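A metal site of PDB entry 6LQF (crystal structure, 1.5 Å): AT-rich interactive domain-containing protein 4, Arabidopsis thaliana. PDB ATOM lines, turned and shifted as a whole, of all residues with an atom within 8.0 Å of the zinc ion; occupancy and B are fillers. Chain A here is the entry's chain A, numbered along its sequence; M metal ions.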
ATOM      1  N   CYS A 133     -31.738 -19.644 -31.233  1.00  0.00           N
ATOM      2  CA  CYS A 133     -30.816 -20.675 -30.754  1.00  0.00           C
ATOM      3  C   CYS A 133     -29.464 -20.025 -30.425  1.00  0.00           C
ATOM      4  O   CYS A 133     -29.214 -18.873 -30.738  1.00  0.00           O
ATOM      5  CB  CYS A 133     -30.624 -21.774 -31.797  1.00  0.00           C
ATOM      6  SG  CYS A 133     -29.720 -21.254 -33.290  1.00  0.00           S
ATOM      7  N   CYS A 134     -28.625 -20.779 -29.740  1.00  0.00           N
ATOM      8  CA  CYS A 134     -27.250 -20.373 -29.436  1.00  0.00           C
ATOM      9  C   CYS A 134     -26.425 -20.227 -30.706  1.00  0.00           C
ATOM     10  O   CYS A 134     -26.401 -21.120 -31.540  1.00  0.00           O
ATOM     11  CB  CYS A 134     -26.607 -21.442 -28.501  1.00  0.00           C
ATOM     12  SG  CYS A 134     -24.882 -21.120 -28.129  1.00  0.00           S
ATOM     13  N   LEU A 135     -25.733 -19.093 -30.834  1.00  0.00           N
ATOM     14  CA  LEU A 135     -24.971 -18.808 -32.045  1.00  0.00           C
ATOM     15  C   LEU A 135     -23.802 -19.754 -32.153  1.00  0.00           C
ATOM     16  O   LEU A 135     -23.270 -19.926 -33.258  1.00  0.00           O
ATOM     17  CB  LEU A 135     -24.508 -17.333 -32.062  1.00  0.00           C
ATOM     18  CG  LEU A 135     -23.555 -16.871 -30.938  1.00  0.00           C
ATOM     19  CD1 LEU A 135     -22.088 -17.029 -31.310  1.00  0.00           C
ATOM     20  CD2 LEU A 135     -23.819 -15.410 -30.549  1.00  0.00           C
ATOM     21  N   ILE A 136     -23.374 -20.299 -31.020  1.00  0.00           N
ATOM     22  CA  ILE A 136     -22.240 -21.278 -31.046  1.00  0.00           C
ATOM     23  C   ILE A 136     -22.687 -22.687 -31.350  1.00  0.00           C
ATOM     24  O   ILE A 136     -22.253 -23.273 -32.350  1.00  0.00           O
ATOM     25  CB  ILE A 136     -21.469 -21.267 -29.710  1.00  0.00           C
ATOM     26  CG1 ILE A 136     -20.875 -19.868 -29.508  1.00  0.00           C
ATOM     27  CG2 ILE A 136     -20.349 -22.314 -29.719  1.00  0.00           C
ATOM     28  CD1 ILE A 136     -20.422 -19.548 -28.074  1.00  0.00           C
ATOM     29  N   CYS A 137     -23.547 -23.263 -30.506  1.00  0.00           N
ATOM     30  CA  CYS A 137     -23.935 -24.689 -30.660  1.00  0.00           C
ATOM     31  C   CYS A 137     -25.200 -24.964 -31.445  1.00  0.00           C
ATOM     32  O   CYS A 137     -25.526 -26.102 -31.711  1.00  0.00           O
ATOM     33  CB  CYS A 137     -24.083 -25.348 -29.303  1.00  0.00           C
ATOM     34  SG  CYS A 137     -25.609 -24.869 -28.405  1.00  0.00           S
ATOM     35  N   ARG A 138     -25.972 -23.910 -31.729  1.00  0.00           N
ATOM     36  CA  ARG A 138     -27.147 -23.937 -32.608  1.00  0.00           C
ATOM     37  C   ARG A 138     -28.332 -24.678 -31.976  1.00  0.00           C
ATOM     38  O   ARG A 138     -29.251 -25.102 -32.685  1.00  0.00           O
ATOM     39  CB  ARG A 138     -26.816 -24.545 -33.985  1.00  0.00           C
ATOM     40  CG  ARG A 138     -25.476 -24.148 -34.595  1.00  0.00           C
ATOM     41  CD  ARG A 138     -25.303 -22.633 -34.819  1.00  0.00           C
ATOM     42  NE  ARG A 138     -26.480 -22.020 -35.418  1.00  0.00           N
ATOM     43  CZ  ARG A 138     -26.512 -20.772 -35.897  1.00  0.00           C
ATOM     44  NH1 ARG A 138     -25.421 -20.004 -35.878  1.00  0.00           N
ATOM     45  NH2 ARG A 138     -27.642 -20.291 -36.417  1.00  0.00           N
ATOM     46  N   SER A 139     -28.317 -24.821 -30.649  1.00  0.00           N
ATOM     47  CA  SER A 139     -29.454 -25.427 -29.949  1.00  0.00           C
ATOM     48  C   SER A 139     -30.080 -24.438 -28.970  1.00  0.00           C
ATOM     49  O   SER A 139     -29.526 -23.364 -28.723  1.00  0.00           O
ATOM     50  CB  SER A 139     -28.996 -26.675 -29.188  1.00  0.00           C
ATOM     51  OG  SER A 139     -28.619 -26.338 -27.860  1.00  0.00           O
ATOM     52  N   SER A 140     -31.232 -24.825 -28.395  1.00  0.00           N
ATOM     53  CA  SER A 140     -31.947 -23.967 -27.443  1.00  0.00           C
ATOM     54  C   SER A 140     -31.911 -24.480 -26.016  1.00  0.00           C
ATOM     55  O   SER A 140     -32.792 -24.128 -25.208  1.00  0.00           O
ATOM     56  CB  SER A 140     -33.395 -23.807 -27.870  1.00  0.00           C
ATOM     57  OG  SER A 140     -33.479 -22.989 -29.011  1.00  0.00           O
ATOM     58  N   THR A 141     -30.921 -25.316 -25.715  1.00  0.00           N
ATOM     59  CA  THR A 141     -30.772 -25.956 -24.402  1.00  0.00           C
ATOM     60  C   THR A 141     -30.916 -24.992 -23.242  1.00  0.00           C
ATOM     61  O   THR A 141     -30.480 -23.836 -23.306  1.00  0.00           O
ATOM     62  CB  THR A 141     -29.377 -26.653 -24.304  1.00  0.00           C
ATOM     63  OG1 THR A 141     -29.114 -27.350 -25.519  1.00  0.00           O
ATOM     64  CG2 THR A 141     -29.329 -27.636 -23.137  1.00  0.00           C
ATOM     65  N   ASP A 144     -27.671 -20.696 -18.835  1.00  0.00           N
ATOM     66  CA  ASP A 144     -27.362 -19.276 -18.811  1.00  0.00           C
ATOM     67  C   ASP A 144     -26.982 -18.763 -20.170  1.00  0.00           C
ATOM     68  O   ASP A 144     -26.130 -19.361 -20.806  1.00  0.00           O
ATOM     69  CB  ASP A 144     -26.234 -18.987 -17.832  1.00  0.00           C
ATOM     70  CG  ASP A 144     -26.584 -19.341 -16.384  1.00  0.00           C
ATOM     71  OD1 ASP A 144     -27.786 -19.403 -16.018  1.00  0.00           O
ATOM     72  OD2 ASP A 144     -25.615 -19.507 -15.601  1.00  0.00           O
ATOM     73  N   TRP A 145     -27.549 -17.630 -20.590  1.00  0.00           N
ATOM     74  CA  TRP A 145     -27.239 -17.026 -21.875  1.00  0.00           C
ATOM     75  C   TRP A 145     -26.781 -15.597 -21.745  1.00  0.00           C
ATOM     76  O   TRP A 145     -27.282 -14.849 -20.877  1.00  0.00           O
ATOM     77  CB  TRP A 145     -28.482 -16.980 -22.758  1.00  0.00           C
ATOM     78  CG  TRP A 145     -29.259 -18.248 -23.021  1.00  0.00           C
ATOM     79  CD1 TRP A 145     -30.017 -18.982 -22.136  1.00  0.00           C
ATOM     80  CD2 TRP A 145     -29.427 -18.877 -24.306  1.00  0.00           C
ATOM     81  NE1 TRP A 145     -30.637 -20.011 -22.800  1.00  0.00           N
ATOM     82  CE2 TRP A 145     -30.300 -19.962 -24.139  1.00  0.00           C
ATOM     83  CE3 TRP A 145     -28.966 -18.552 -25.599  1.00  0.00           C
ATOM     84  CZ2 TRP A 145     -30.696 -20.775 -25.211  1.00  0.00           C
ATOM     85  CZ3 TRP A 145     -29.345 -19.359 -26.658  1.00  0.00           C
ATOM     86  CH2 TRP A 145     -30.222 -20.461 -26.457  1.00  0.00           C
ATOM     87  N   TRP A 154     -27.617 -14.486 -29.555  1.00  0.00           N
ATOM     88  CA  TRP A 154     -27.529 -15.018 -28.217  1.00  0.00           C
ATOM     89  C   TRP A 154     -26.645 -16.254 -28.129  1.00  0.00           C
ATOM     90  O   TRP A 154     -26.606 -17.009 -29.063  1.00  0.00           O
ATOM     91  CB  TRP A 154     -28.912 -15.439 -27.745  1.00  0.00           C
ATOM     92  CG  TRP A 154     -29.840 -14.286 -27.358  1.00  0.00           C
ATOM     93  CD1 TRP A 154     -30.758 -13.656 -28.139  1.00  0.00           C
ATOM     94  CD2 TRP A 154     -29.945 -13.716 -26.058  1.00  0.00           C
ATOM     95  NE1 TRP A 154     -31.432 -12.700 -27.400  1.00  0.00           N
ATOM     96  CE2 TRP A 154     -30.979 -12.763 -26.105  1.00  0.00           C
ATOM     97  CE3 TRP A 154     -29.315 -13.994 -24.839  1.00  0.00           C
ATOM     98  CZ2 TRP A 154     -31.331 -12.001 -24.976  1.00  0.00           C
ATOM     99  CZ3 TRP A 154     -29.657 -13.246 -23.733  1.00  0.00           C
ATOM    100  CH2 TRP A 154     -30.683 -12.312 -23.773  1.00  0.00           C
ATOM    101  N   ALA A 155     -25.883 -16.347 -27.053  1.00  0.00           N
ATOM    102  CA  ALA A 155     -24.993 -17.490 -26.831  1.00  0.00           C
ATOM    103  C   ALA A 155     -25.185 -18.072 -25.443  1.00  0.00           C
ATOM    104  O   ALA A 155     -25.360 -17.350 -24.465  1.00  0.00           O
ATOM    105  CB  ALA A 155     -23.544 -17.070 -27.019  1.00  0.00           C
ATOM    106  N   HIS A 156     -25.140 -19.394 -25.311  1.00  0.00           N
ATOM    107  CA  HIS A 156     -24.944 -19.925 -23.977  1.00  0.00           C
ATOM    108  C   HIS A 156     -23.621 -19.477 -23.413  1.00  0.00           C
ATOM    109  O   HIS A 156     -22.571 -19.655 -24.061  1.00  0.00           O
ATOM    110  CB  HIS A 156     -24.861 -21.466 -23.972  1.00  0.00           C
ATOM    111  CG  HIS A 156     -26.123 -22.146 -24.365  1.00  0.00           C
ATOM    112  ND1 HIS A 156     -26.253 -22.848 -25.547  1.00  0.00           N
ATOM    113  CD2 HIS A 156     -27.359 -22.170 -23.783  1.00  0.00           C
ATOM    114  CE1 HIS A 156     -27.453 -23.401 -25.608  1.00  0.00           C
ATOM    115  NE2 HIS A 156     -28.165 -22.955 -24.575  1.00  0.00           N
ATOM    116  N   PHE A 157     -23.611 -19.051 -22.171  1.00  0.00           N
ATOM    117  CA  PHE A 157     -22.365 -18.676 -21.522  1.00  0.00           C
ATOM    118  C   PHE A 157     -21.385 -19.836 -21.530  1.00  0.00           C
ATOM    119  O   PHE A 157     -20.174 -19.645 -21.781  1.00  0.00           O
ATOM    120  CB  PHE A 157     -22.665 -18.217 -20.098  1.00  0.00           C
ATOM    121  CG  PHE A 157     -21.510 -17.568 -19.420  1.00  0.00           C
ATOM    122  CD1 PHE A 157     -21.070 -16.326 -19.856  1.00  0.00           C
ATOM    123  CD2 PHE A 157     -20.905 -18.146 -18.320  1.00  0.00           C
ATOM    124  CE1 PHE A 157     -19.989 -15.693 -19.219  1.00  0.00           C
ATOM    125  CE2 PHE A 157     -19.816 -17.533 -17.677  1.00  0.00           C
ATOM    126  CZ  PHE A 157     -19.374 -16.294 -18.137  1.00  0.00           C
ATOM    127  N   GLY A 158     -21.944 -21.036 -21.312  1.00  0.00           N
ATOM    128  CA  GLY A 158     -21.165 -22.294 -21.259  1.00  0.00           C
ATOM    129  C   GLY A 158     -20.571 -22.689 -22.577  1.00  0.00           C
ATOM    130  O   GLY A 158     -19.642 -23.527 -22.610  1.00  0.00           O
ATOM    131  N   CYS A 159     -21.055 -22.145 -23.681  1.00  0.00           N
ATOM    132  CA  CYS A 159     -20.496 -22.521 -24.991  1.00  0.00           C
ATOM    133  C   CYS A 159     -19.307 -21.630 -25.384  1.00  0.00           C
ATOM    134  O   CYS A 159     -18.687 -21.836 -26.431  1.00  0.00           O
ATOM    135  CB  CYS A 159     -21.568 -22.485 -26.097  1.00  0.00           C
ATOM    136  SG  CYS A 159     -22.748 -23.898 -26.083  1.00  0.00           S
ATOM    137  N   ASP A 160     -19.016 -20.638 -24.568  1.00  0.00           N
ATOM    138  CA  ASP A 160     -17.898 -19.741 -24.857  1.00  0.00           C
ATOM    139  C   ASP A 160     -16.740 -20.175 -23.948  1.00  0.00           C
ATOM    140  O   ASP A 160     -16.770 -19.954 -22.755  1.00  0.00           O
ATOM    141  CB  ASP A 160     -18.313 -18.265 -24.633  1.00  0.00           C
ATOM    142  CG  ASP A 160     -17.263 -17.310 -25.100  1.00  0.00           C
ATOM    143  OD1 ASP A 160     -16.075 -17.718 -25.263  1.00  0.00           O
ATOM    144  OD2 ASP A 160     -17.616 -16.123 -25.321  1.00  0.00           O
HETATM  145 ZN    ZN M   1     -24.728 -23.174 -26.945  1.00  0.00          ZN
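A ring nitrogen (NE2) of His 156 sits at hydrogen-bond distance from the backbone carbonyl oxygen (O) of Thr 141, at 2.8 Å.
SG of Cys 137 sits close to OG of Ser 139.
N of Ile 136 lies close to SG of Cys 134 (3.4 Å).
O of Ser 139 is in hydrogen-bond range of N of Cys 134 (2.9 Å).
Four residues have an atom within 4 Å of the zinc ion: Cys 134, Cys 137, His 156 and Cys 159.
The nearest printed residue that does not touch the zinc ion is Ile 136 (4.7 Å).
ND1 of His 156 binds the zinc ion, at 2.1 Å.
SG of Cys 159 is bound to the zinc ion.
The zinc ion is bound by SG of Cys 134 (2.4 Å).
The zinc ion is bound by SG of Cys 137, at 2.4 Å.
The zinc ion has four donor atoms within binding distance.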
